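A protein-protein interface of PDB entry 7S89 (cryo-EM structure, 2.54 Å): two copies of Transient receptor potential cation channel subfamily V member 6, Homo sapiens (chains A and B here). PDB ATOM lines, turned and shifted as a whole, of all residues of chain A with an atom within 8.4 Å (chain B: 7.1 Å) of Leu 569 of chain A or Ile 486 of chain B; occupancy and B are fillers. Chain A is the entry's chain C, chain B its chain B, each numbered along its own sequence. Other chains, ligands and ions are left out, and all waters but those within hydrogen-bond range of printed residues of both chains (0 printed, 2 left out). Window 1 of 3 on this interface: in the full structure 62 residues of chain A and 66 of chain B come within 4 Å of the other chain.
The backbone carbonyl oxygen of Met 485 of chain B sits at hydrogen-bond distance from the backbone NH of Leu 490 of chain B (2.9 Å). The backbone NH (N) of Met 491 of chain B sits at hydrogen-bond distance from the backbone carbonyl oxygen (O) of Ile 486 of chain B (3.0 Å). The side-chain amide nitrogen of Asn 572 of chain A lies within hydrogen-bond range of the backbone carbonyl oxygen of Leu 568 of chain A. O of Ile 564 of chain A sits at hydrogen-bond distance from N of Leu 569 of chain A (3.1 Å). O of Ala 563 of chain A sits at hydrogen-bond distance from N of Leu 568 of chain A, 3.1 Å away.
Printed residues of chain A that touch a printed residue of chain B: Phe 493, Ile 564, Leu 568, Leu 569 and Leu 573. Hydrophobic or aromatic side chains of chain B within 4 Å of the printed part of chain A: Phe 478, Met 481, Ile 482, Met 485, Ile 486, Leu 490, Leu 574 and Met 578.
Of chain B, only Ile 482, Met 485, Ile 486 and Leu 490 come within 4 Å of Leu 569 of chain A. Ile 486 of chain B touches just one residue of chain A: Leu 569. No residue of chain A comes within 4 Å of Phe 487 of chain B. Of the printed residues of chain A, Phe 478 of chain B touches Phe 493. Printed residues of chain A within 4 Å of Met 578 of chain B: Leu 568. Lys 484 of chain B touches none of the printed residues of chain A. Gln 483 of chain B touches none of the printed residues of chain A.
Position printed for both chains: 574. Of the 11 pairs that touch across the chains among the printed residues, none has its exchanged pair printed and touching as well.
CD1 of Phe 493 of chain A touches CD2 of Phe 478 of chain B (3.5 Å). Ile 564 of chain A touches Leu 490 of chain B. CD2 of Leu 574 of chain B touches CD1 of Leu 568 of chain A (3.8 Å). Leu 569 of chain A touches Ile 482 of chain B. CD1 of Leu 569 of chain A touches CB of Met 485 of chain B (3.6 Å). Ile 486 of chain B touches Leu 569 of chain A. CD1 of Leu 490 of chain B touches CD1 of Leu 569 of chain A, at 3.8 Å. CD2 of Leu 573 of chain A touches SD of Met 481 of chain B, 3.8 Å away. Leu 573 of chain A touches Ile 482 of chain B. Met 485 of chain B touches Leu 573 of chain A.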
ATOM      1  N   PHE A 493      23.687  -4.425  30.092  1.00  0.00           N
ATOM      2  CA  PHE A 493      23.885  -3.115  29.501  1.00  0.00           C
ATOM      3  C   PHE A 493      25.278  -2.938  28.907  1.00  0.00           C
ATOM      4  O   PHE A 493      25.534  -1.913  28.279  1.00  0.00           O
ATOM      5  CB  PHE A 493      23.573  -2.046  30.555  1.00  0.00           C
ATOM      6  CG  PHE A 493      23.374  -0.667  29.999  1.00  0.00           C
ATOM      7  CD1 PHE A 493      22.291  -0.383  29.196  1.00  0.00           C
ATOM      8  CD2 PHE A 493      24.249   0.346  30.318  1.00  0.00           C
ATOM      9  CE1 PHE A 493      22.089   0.882  28.697  1.00  0.00           C
ATOM     10  CE2 PHE A 493      24.062   1.621  29.817  1.00  0.00           C
ATOM     11  CZ  PHE A 493      22.976   1.886  29.005  1.00  0.00           C
ATOM     12  N   MET A 497      26.724  -0.607  25.708  1.00  0.00           N
ATOM     13  CA  MET A 497      27.926   0.190  25.913  1.00  0.00           C
ATOM     14  C   MET A 497      29.026  -0.182  24.934  1.00  0.00           C
ATOM     15  O   MET A 497      29.726   0.701  24.432  1.00  0.00           O
ATOM     16  CB  MET A 497      28.446   0.029  27.330  1.00  0.00           C
ATOM     17  CG  MET A 497      27.645   0.714  28.368  1.00  0.00           C
ATOM     18  SD  MET A 497      28.516   0.565  29.924  1.00  0.00           S
ATOM     19  CE  MET A 497      27.487   1.595  30.907  1.00  0.00           C
ATOM     20  N   PHE A 537      34.648   6.880  28.153  1.00  0.00           N
ATOM     21  CA  PHE A 537      33.297   6.505  28.541  1.00  0.00           C
ATOM     22  C   PHE A 537      33.105   6.628  30.046  1.00  0.00           C
ATOM     23  O   PHE A 537      32.094   7.162  30.513  1.00  0.00           O
ATOM     24  CB  PHE A 537      33.012   5.062  28.113  1.00  0.00           C
ATOM     25  CG  PHE A 537      31.578   4.666  28.228  1.00  0.00           C
ATOM     26  CD1 PHE A 537      30.746   4.785  27.152  1.00  0.00           C
ATOM     27  CD2 PHE A 537      31.042   4.220  29.426  1.00  0.00           C
ATOM     28  CE1 PHE A 537      29.409   4.464  27.256  1.00  0.00           C
ATOM     29  CE2 PHE A 537      29.732   3.929  29.539  1.00  0.00           C
ATOM     30  CZ  PHE A 537      28.911   4.042  28.450  1.00  0.00           C
ATOM     31  N   ALA A 561      29.476  14.722  20.733  1.00  0.00           N
ATOM     32  CA  ALA A 561      28.427  13.719  20.642  1.00  0.00           C
ATOM     33  C   ALA A 561      28.698  12.556  21.577  1.00  0.00           C
ATOM     34  O   ALA A 561      27.774  12.010  22.178  1.00  0.00           O
ATOM     35  CB  ALA A 561      28.299  13.223  19.210  1.00  0.00           C
ATOM     36  N   PHE A 562      29.965  12.166  21.701  1.00  0.00           N
ATOM     37  CA  PHE A 562      30.355  11.106  22.615  1.00  0.00           C
ATOM     38  C   PHE A 562      30.139  11.514  24.059  1.00  0.00           C
ATOM     39  O   PHE A 562      29.666  10.717  24.862  1.00  0.00           O
ATOM     40  CB  PHE A 562      31.816  10.732  22.381  1.00  0.00           C
ATOM     41  CG  PHE A 562      32.303   9.637  23.252  1.00  0.00           C
ATOM     42  CD1 PHE A 562      31.940   8.337  23.005  1.00  0.00           C
ATOM     43  CD2 PHE A 562      33.136   9.902  24.321  1.00  0.00           C
ATOM     44  CE1 PHE A 562      32.387   7.328  23.799  1.00  0.00           C
ATOM     45  CE2 PHE A 562      33.577   8.894  25.117  1.00  0.00           C
ATOM     46  CZ  PHE A 562      33.205   7.605  24.850  1.00  0.00           C
ATOM     47  N   ALA A 563      30.475  12.751  24.405  1.00  0.00           N
ATOM     48  CA  ALA A 563      30.356  13.206  25.785  1.00  0.00           C
ATOM     49  C   ALA A 563      28.908  13.239  26.242  1.00  0.00           C
ATOM     50  O   ALA A 563      28.613  12.978  27.411  1.00  0.00           O
ATOM     51  CB  ALA A 563      30.985  14.580  25.925  1.00  0.00           C
ATOM     52  N   ILE A 564      27.992  13.531  25.326  1.00  0.00           N
ATOM     53  CA  ILE A 564      26.578  13.565  25.663  1.00  0.00           C
ATOM     54  C   ILE A 564      26.007  12.155  25.769  1.00  0.00           C
ATOM     55  O   ILE A 564      25.372  11.815  26.768  1.00  0.00           O
ATOM     56  CB  ILE A 564      25.812  14.422  24.644  1.00  0.00           C
ATOM     57  CG1 ILE A 564      26.254  15.874  24.759  1.00  0.00           C
ATOM     58  CG2 ILE A 564      24.332  14.305  24.855  1.00  0.00           C
ATOM     59  CD1 ILE A 564      25.809  16.727  23.629  1.00  0.00           C
ATOM     60  N   ILE A 565      26.205  11.314  24.750  1.00  0.00           N
ATOM     61  CA  ILE A 565      25.532  10.017  24.784  1.00  0.00           C
ATOM     62  C   ILE A 565      26.212   9.075  25.766  1.00  0.00           C
ATOM     63  O   ILE A 565      25.546   8.337  26.489  1.00  0.00           O
ATOM     64  CB  ILE A 565      25.390   9.383  23.378  1.00  0.00           C
ATOM     65  CG1 ILE A 565      24.524   8.125  23.475  1.00  0.00           C
ATOM     66  CG2 ILE A 565      26.699   8.992  22.741  1.00  0.00           C
ATOM     67  CD1 ILE A 565      24.133   7.524  22.179  1.00  0.00           C
ATOM     68  N   ALA A 566      27.527   9.137  25.892  1.00  0.00           N
ATOM     69  CA  ALA A 566      28.232   8.127  26.658  1.00  0.00           C
ATOM     70  C   ALA A 566      28.449   8.554  28.100  1.00  0.00           C
ATOM     71  O   ALA A 566      27.996   7.874  29.018  1.00  0.00           O
ATOM     72  CB  ALA A 566      29.557   7.794  25.979  1.00  0.00           C
ATOM     73  N   THR A 567      29.130   9.673  28.317  1.00  0.00           N
ATOM     74  CA  THR A 567      29.499  10.038  29.676  1.00  0.00           C
ATOM     75  C   THR A 567      28.303  10.581  30.442  1.00  0.00           C
ATOM     76  O   THR A 567      28.105  10.233  31.607  1.00  0.00           O
ATOM     77  CB  THR A 567      30.638  11.058  29.669  1.00  0.00           C
ATOM     78  OG1 THR A 567      30.144  12.326  29.238  1.00  0.00           O
ATOM     79  CG2 THR A 567      31.692  10.629  28.709  1.00  0.00           C
ATOM     80  N   LEU A 568      27.500  11.433  29.815  1.00  0.00           N
ATOM     81  CA  LEU A 568      26.286  11.893  30.465  1.00  0.00           C
ATOM     82  C   LEU A 568      25.237  10.808  30.555  1.00  0.00           C
ATOM     83  O   LEU A 568      24.858  10.399  31.648  1.00  0.00           O
ATOM     84  CB  LEU A 568      25.662  13.076  29.734  1.00  0.00           C
ATOM     85  CG  LEU A 568      25.828  14.477  30.268  1.00  0.00           C
ATOM     86  CD1 LEU A 568      25.019  15.396  29.385  1.00  0.00           C
ATOM     87  CD2 LEU A 568      25.275  14.469  31.654  1.00  0.00           C
ATOM     88  N   LEU A 569      24.765  10.333  29.416  1.00  0.00           N
ATOM     89  CA  LEU A 569      23.506   9.615  29.397  1.00  0.00           C
ATOM     90  C   LEU A 569      23.657   8.148  29.772  1.00  0.00           C
ATOM     91  O   LEU A 569      23.014   7.686  30.711  1.00  0.00           O
ATOM     92  CB  LEU A 569      22.865   9.781  28.024  1.00  0.00           C
ATOM     93  CG  LEU A 569      21.453   9.269  27.871  1.00  0.00           C
ATOM     94  CD1 LEU A 569      20.812  10.290  27.058  1.00  0.00           C
ATOM     95  CD2 LEU A 569      21.406   7.944  27.147  1.00  0.00           C
ATOM     96  N   MET A 570      24.477   7.401  29.035  1.00  0.00           N
ATOM     97  CA  MET A 570      24.508   5.956  29.220  1.00  0.00           C
ATOM     98  C   MET A 570      25.247   5.571  30.489  1.00  0.00           C
ATOM     99  O   MET A 570      24.936   4.549  31.103  1.00  0.00           O
ATOM    100  CB  MET A 570      25.136   5.280  28.010  1.00  0.00           C
ATOM    101  CG  MET A 570      24.293   5.370  26.771  1.00  0.00           C
ATOM    102  SD  MET A 570      25.068   4.626  25.340  1.00  0.00           S
ATOM    103  CE  MET A 570      24.861   2.901  25.719  1.00  0.00           C
ATOM    104  N   LEU A 571      26.232   6.371  30.893  1.00  0.00           N
ATOM    105  CA  LEU A 571      26.946   6.088  32.127  1.00  0.00           C
ATOM    106  C   LEU A 571      26.054   6.314  33.337  1.00  0.00           C
ATOM    107  O   LEU A 571      26.081   5.534  34.289  1.00  0.00           O
ATOM    108  CB  LEU A 571      28.202   6.946  32.218  1.00  0.00           C
ATOM    109  CG  LEU A 571      29.100   6.615  33.405  1.00  0.00           C
ATOM    110  CD1 LEU A 571      29.602   5.211  33.257  1.00  0.00           C
ATOM    111  CD2 LEU A 571      30.247   7.594  33.518  1.00  0.00           C
ATOM    112  N   ASN A 572      25.235   7.356  33.308  1.00  0.00           N
ATOM    113  CA  ASN A 572      24.350   7.611  34.434  1.00  0.00           C
ATOM    114  C   ASN A 572      23.117   6.730  34.376  1.00  0.00           C
ATOM    115  O   ASN A 572      22.444   6.536  35.388  1.00  0.00           O
ATOM    116  CB  ASN A 572      23.982   9.082  34.471  1.00  0.00           C
ATOM    117  CG  ASN A 572      25.148   9.942  34.866  1.00  0.00           C
ATOM    118  OD1 ASN A 572      25.822   9.663  35.848  1.00  0.00           O
ATOM    119  ND2 ASN A 572      25.436  10.950  34.070  1.00  0.00           N
ATOM    120  N   LEU A 573      22.807   6.194  33.200  1.00  0.00           N
ATOM    121  CA  LEU A 573      21.736   5.217  33.077  1.00  0.00           C
ATOM    122  C   LEU A 573      22.106   3.927  33.799  1.00  0.00           C
ATOM    123  O   LEU A 573      21.267   3.315  34.460  1.00  0.00           O
ATOM    124  CB  LEU A 573      21.455   4.959  31.598  1.00  0.00           C
ATOM    125  CG  LEU A 573      20.141   4.392  31.067  1.00  0.00           C
ATOM    126  CD1 LEU A 573      20.001   4.769  29.623  1.00  0.00           C
ATOM    127  CD2 LEU A 573      20.047   2.940  31.170  1.00  0.00           C
ATOM    128  N   LEU A 574      23.361   3.495  33.659  1.00  0.00           N
ATOM    129  CA  LEU A 574      23.835   2.292  34.335  1.00  0.00           C
ATOM    130  C   LEU A 574      23.881   2.481  35.840  1.00  0.00           C
ATOM    131  O   LEU A 574      23.530   1.574  36.599  1.00  0.00           O
ATOM    132  CB  LEU A 574      25.224   1.907  33.827  1.00  0.00           C
ATOM    133  CG  LEU A 574      25.766   0.620  34.459  1.00  0.00           C
ATOM    134  CD1 LEU A 574      25.034  -0.597  33.943  1.00  0.00           C
ATOM    135  CD2 LEU A 574      27.257   0.447  34.351  1.00  0.00           C
ATOM    136  N   ILE A 575      24.332   3.651  36.286  1.00  0.00           N
ATOM    137  CA  ILE A 575      24.385   3.961  37.709  1.00  0.00           C
ATOM    138  C   ILE A 575      22.980   4.014  38.299  1.00  0.00           C
ATOM    139  O   ILE A 575      22.755   3.585  39.435  1.00  0.00           O
ATOM    140  CB  ILE A 575      25.166   5.275  37.918  1.00  0.00           C
ATOM    141  CG1 ILE A 575      26.610   5.098  37.458  1.00  0.00           C
ATOM    142  CG2 ILE A 575      25.182   5.699  39.348  1.00  0.00           C
ATOM    143  CD1 ILE A 575      27.367   6.383  37.329  1.00  0.00           C
ATOM    144  N   ALA A 576      22.007   4.488  37.519  1.00  0.00           N
ATOM    145  CA  ALA A 576      20.617   4.468  37.964  1.00  0.00           C
ATOM    146  C   ALA A 576      20.086   3.046  38.092  1.00  0.00           C
ATOM    147  O   ALA A 576      19.271   2.763  38.974  1.00  0.00           O
ATOM    148  CB  ALA A 576      19.744   5.278  37.012  1.00  0.00           C
ATOM    149  N   PHE B 478      15.949  -0.703  27.208  1.00  0.00           N
ATOM    150  CA  PHE B 478      17.079   0.198  27.424  1.00  0.00           C
ATOM    151  C   PHE B 478      17.117   1.298  26.377  1.00  0.00           C
ATOM    152  O   PHE B 478      17.472   2.439  26.682  1.00  0.00           O
ATOM    153  CB  PHE B 478      18.398  -0.562  27.393  1.00  0.00           C
ATOM    154  CG  PHE B 478      18.641  -1.425  28.580  1.00  0.00           C
ATOM    155  CD1 PHE B 478      17.972  -1.208  29.768  1.00  0.00           C
ATOM    156  CD2 PHE B 478      19.531  -2.479  28.497  1.00  0.00           C
ATOM    157  CE1 PHE B 478      18.184  -2.024  30.849  1.00  0.00           C
ATOM    158  CE2 PHE B 478      19.757  -3.288  29.579  1.00  0.00           C
ATOM    159  CZ  PHE B 478      19.091  -3.058  30.757  1.00  0.00           C
ATOM    160  N   ILE B 480      14.537   2.477  24.806  1.00  0.00           N
ATOM    161  CA  ILE B 480      13.434   3.383  25.106  1.00  0.00           C
ATOM    162  C   ILE B 480      13.852   4.383  26.179  1.00  0.00           C
ATOM    163  O   ILE B 480      13.466   5.556  26.133  1.00  0.00           O
ATOM    164  CB  ILE B 480      12.181   2.582  25.512  1.00  0.00           C
ATOM    165  CG1 ILE B 480      11.774   1.638  24.386  1.00  0.00           C
ATOM    166  CG2 ILE B 480      11.007   3.491  25.811  1.00  0.00           C
ATOM    167  CD1 ILE B 480      10.698   0.690  24.770  1.00  0.00           C
ATOM    168  N   MET B 481      14.673   3.943  27.139  1.00  0.00           N
ATOM    169  CA  MET B 481      15.255   4.862  28.115  1.00  0.00           C
ATOM    170  C   MET B 481      16.138   5.900  27.446  1.00  0.00           C
ATOM    171  O   MET B 481      16.079   7.078  27.792  1.00  0.00           O
ATOM    172  CB  MET B 481      16.078   4.108  29.154  1.00  0.00           C
ATOM    173  CG  MET B 481      15.302   3.236  30.068  1.00  0.00           C
ATOM    174  SD  MET B 481      16.307   2.388  31.274  1.00  0.00           S
ATOM    175  CE  MET B 481      15.085   1.341  32.031  1.00  0.00           C
ATOM    176  N   ILE B 482      16.946   5.482  26.473  1.00  0.00           N
ATOM    177  CA  ILE B 482      17.848   6.400  25.788  1.00  0.00           C
ATOM    178  C   ILE B 482      17.065   7.423  24.977  1.00  0.00           C
ATOM    179  O   ILE B 482      17.401   8.613  24.967  1.00  0.00           O
ATOM    180  CB  ILE B 482      18.838   5.605  24.918  1.00  0.00           C
ATOM    181  CG1 ILE B 482      19.723   4.733  25.799  1.00  0.00           C
ATOM    182  CG2 ILE B 482      19.693   6.519  24.072  1.00  0.00           C
ATOM    183  CD1 ILE B 482      20.524   3.728  25.027  1.00  0.00           C
ATOM    184  N   GLN B 483      15.986   6.983  24.320  1.00  0.00           N
ATOM    185  CA  GLN B 483      15.160   7.903  23.549  1.00  0.00           C
ATOM    186  C   GLN B 483      14.459   8.911  24.449  1.00  0.00           C
ATOM    187  O   GLN B 483      14.394  10.098  24.126  1.00  0.00           O
ATOM    188  CB  GLN B 483      14.117   7.143  22.738  1.00  0.00           C
ATOM    189  CG  GLN B 483      13.393   8.037  21.767  1.00  0.00           C
ATOM    190  CD  GLN B 483      12.188   7.397  21.143  1.00  0.00           C
ATOM    191  OE1 GLN B 483      11.714   6.366  21.600  1.00  0.00           O
ATOM    192  NE2 GLN B 483      11.706   7.984  20.059  1.00  0.00           N
ATOM    193  N   LYS B 484      13.937   8.460  25.585  1.00  0.00           N
ATOM    194  CA  LYS B 484      13.227   9.362  26.476  1.00  0.00           C
ATOM    195  C   LYS B 484      14.163  10.207  27.326  1.00  0.00           C
ATOM    196  O   LYS B 484      13.716  11.188  27.918  1.00  0.00           O
ATOM    197  CB  LYS B 484      12.268   8.572  27.361  1.00  0.00           C
ATOM    198  CG  LYS B 484      11.135   7.965  26.589  1.00  0.00           C
ATOM    199  CD  LYS B 484      10.161   7.250  27.481  1.00  0.00           C
ATOM    200  CE  LYS B 484       9.039   6.640  26.659  1.00  0.00           C
ATOM    201  NZ  LYS B 484       8.046   5.945  27.518  1.00  0.00           N
ATOM    202  N   MET B 485      15.439   9.846  27.412  1.00  0.00           N
ATOM    203  CA  MET B 485      16.410  10.740  28.024  1.00  0.00           C
ATOM    204  C   MET B 485      16.956  11.755  27.031  1.00  0.00           C
ATOM    205  O   MET B 485      17.343  12.853  27.434  1.00  0.00           O
ATOM    206  CB  MET B 485      17.560   9.945  28.635  1.00  0.00           C
ATOM    207  CG  MET B 485      17.217   9.185  29.877  1.00  0.00           C
ATOM    208  SD  MET B 485      18.543   8.089  30.364  1.00  0.00           S
ATOM    209  CE  MET B 485      17.656   7.052  31.508  1.00  0.00           C
ATOM    210  N   ILE B 486      16.999  11.419  25.743  1.00  0.00           N
ATOM    211  CA  ILE B 486      17.459  12.376  24.742  1.00  0.00           C
ATOM    212  C   ILE B 486      16.345  13.338  24.363  1.00  0.00           C
ATOM    213  O   ILE B 486      16.483  14.554  24.523  1.00  0.00           O
ATOM    214  CB  ILE B 486      18.048  11.651  23.516  1.00  0.00           C
ATOM    215  CG1 ILE B 486      19.414  11.119  23.898  1.00  0.00           C
ATOM    216  CG2 ILE B 486      18.203  12.582  22.336  1.00  0.00           C
ATOM    217  CD1 ILE B 486      20.130  10.311  22.913  1.00  0.00           C
ATOM    218  N   PHE B 487      15.222  12.817  23.888  1.00  0.00           N
ATOM    219  CA  PHE B 487      14.140  13.660  23.400  1.00  0.00           C
ATOM    220  C   PHE B 487      13.203  14.105  24.509  1.00  0.00           C
ATOM    221  O   PHE B 487      12.254  14.848  24.251  1.00  0.00           O
ATOM    222  CB  PHE B 487      13.393  12.920  22.293  1.00  0.00           C
ATOM    223  CG  PHE B 487      14.267  12.600  21.126  1.00  0.00           C
ATOM    224  CD1 PHE B 487      14.584  13.577  20.206  1.00  0.00           C
ATOM    225  CD2 PHE B 487      14.825  11.343  20.982  1.00  0.00           C
ATOM    226  CE1 PHE B 487      15.417  13.301  19.150  1.00  0.00           C
ATOM    227  CE2 PHE B 487      15.657  11.058  19.931  1.00  0.00           C
ATOM    228  CZ  PHE B 487      15.951  12.036  19.010  1.00  0.00           C
ATOM    229  N   GLY B 488      13.481  13.695  25.730  1.00  0.00           N
ATOM    230  CA  GLY B 488      12.826  14.174  26.919  1.00  0.00           C
ATOM    231  C   GLY B 488      13.770  15.111  27.634  1.00  0.00           C
ATOM    232  O   GLY B 488      13.791  16.306  27.349  1.00  0.00           O
ATOM    233  N   ASP B 489      14.547  14.552  28.564  1.00  0.00           N
ATOM    234  CA  ASP B 489      15.330  15.328  29.521  1.00  0.00           C
ATOM    235  C   ASP B 489      16.376  16.210  28.849  1.00  0.00           C
ATOM    236  O   ASP B 489      16.554  17.366  29.235  1.00  0.00           O
ATOM    237  CB  ASP B 489      15.992  14.372  30.502  1.00  0.00           C
ATOM    238  CG  ASP B 489      14.988  13.566  31.267  1.00  0.00           C
ATOM    239  OD1 ASP B 489      13.881  14.077  31.506  1.00  0.00           O
ATOM    240  OD2 ASP B 489      15.289  12.410  31.611  1.00  0.00           O
ATOM    241  N   LEU B 490      17.077  15.684  27.842  1.00  0.00           N
ATOM    242  CA  LEU B 490      18.124  16.473  27.202  1.00  0.00           C
ATOM    243  C   LEU B 490      17.567  17.627  26.384  1.00  0.00           C
ATOM    244  O   LEU B 490      18.057  18.745  26.513  1.00  0.00           O
ATOM    245  CB  LEU B 490      19.025  15.612  26.332  1.00  0.00           C
ATOM    246  CG  LEU B 490      20.152  14.906  27.054  1.00  0.00           C
ATOM    247  CD1 LEU B 490      20.842  14.000  26.082  1.00  0.00           C
ATOM    248  CD2 LEU B 490      21.102  15.955  27.574  1.00  0.00           C
ATOM    249  N   MET B 491      16.544  17.392  25.560  1.00  0.00           N
ATOM    250  CA  MET B 491      16.023  18.464  24.713  1.00  0.00           C
ATOM    251  C   MET B 491      15.334  19.556  25.524  1.00  0.00           C
ATOM    252  O   MET B 491      15.238  20.700  25.074  1.00  0.00           O
ATOM    253  CB  MET B 491      15.063  17.907  23.665  1.00  0.00           C
ATOM    254  CG  MET B 491      15.720  17.055  22.603  1.00  0.00           C
ATOM    255  SD  MET B 491      17.003  17.915  21.673  1.00  0.00           S
ATOM    256  CE  MET B 491      16.018  19.065  20.717  1.00  0.00           C
ATOM    257  N   ARG B 492      14.854  19.233  26.719  1.00  0.00           N
ATOM    258  CA  ARG B 492      14.257  20.265  27.554  1.00  0.00           C
ATOM    259  C   ARG B 492      15.322  21.075  28.272  1.00  0.00           C
ATOM    260  O   ARG B 492      15.224  22.301  28.357  1.00  0.00           O
ATOM    261  CB  ARG B 492      13.293  19.640  28.555  1.00  0.00           C
ATOM    262  CG  ARG B 492      12.094  19.015  27.911  1.00  0.00           C
ATOM    263  CD  ARG B 492      11.173  18.412  28.937  1.00  0.00           C
ATOM    264  NE  ARG B 492      11.771  17.312  29.672  1.00  0.00           N
ATOM    265  CZ  ARG B 492      11.179  16.705  30.693  1.00  0.00           C
ATOM    266  NH1 ARG B 492       9.977  17.098  31.084  1.00  0.00           N
ATOM    267  NH2 ARG B 492      11.781  15.704  31.315  1.00  0.00           N
ATOM    268  N   LEU B 574      20.354  17.409  35.886  1.00  0.00           N
ATOM    269  CA  LEU B 574      20.031  16.613  34.708  1.00  0.00           C
ATOM    270  C   LEU B 574      20.095  15.126  35.007  1.00  0.00           C
ATOM    271  O   LEU B 574      19.254  14.354  34.539  1.00  0.00           O
ATOM    272  CB  LEU B 574      20.988  16.942  33.563  1.00  0.00           C
ATOM    273  CG  LEU B 574      20.676  16.176  32.272  1.00  0.00           C
ATOM    274  CD1 LEU B 574      19.416  16.690  31.616  1.00  0.00           C
ATOM    275  CD2 LEU B 574      21.815  16.111  31.290  1.00  0.00           C
ATOM    276  N   MET B 578      17.226  12.232  34.583  1.00  0.00           N
ATOM    277  CA  MET B 578      17.375  11.024  33.788  1.00  0.00           C
ATOM    278  C   MET B 578      17.212   9.784  34.644  1.00  0.00           C
ATOM    279  O   MET B 578      16.786   8.739  34.150  1.00  0.00           O
ATOM    280  CB  MET B 578      18.725  11.019  33.084  1.00  0.00           C
ATOM    281  CG  MET B 578      18.887  12.081  32.017  1.00  0.00           C
ATOM    282  SD  MET B 578      20.406  11.879  31.080  1.00  0.00           S
ATOM    283  CE  MET B 578      21.631  12.381  32.272  1.00  0.00           C
ATOM    284  N   THR B 581      13.516   9.389  34.549  1.00  0.00           N
ATOM    285  CA  THR B 581      13.158   8.732  33.295  1.00  0.00           C
ATOM    286  C   THR B 581      13.480   7.243  33.337  1.00  0.00           C
ATOM    287  O   THR B 581      12.679   6.419  32.882  1.00  0.00           O
ATOM    288  CB  THR B 581      13.889   9.407  32.135  1.00  0.00           C
ATOM    289  OG1 THR B 581      13.491  10.775  32.053  1.00  0.00           O
ATOM    290  CG2 THR B 581      13.600   8.725  30.821  1.00  0.00           C
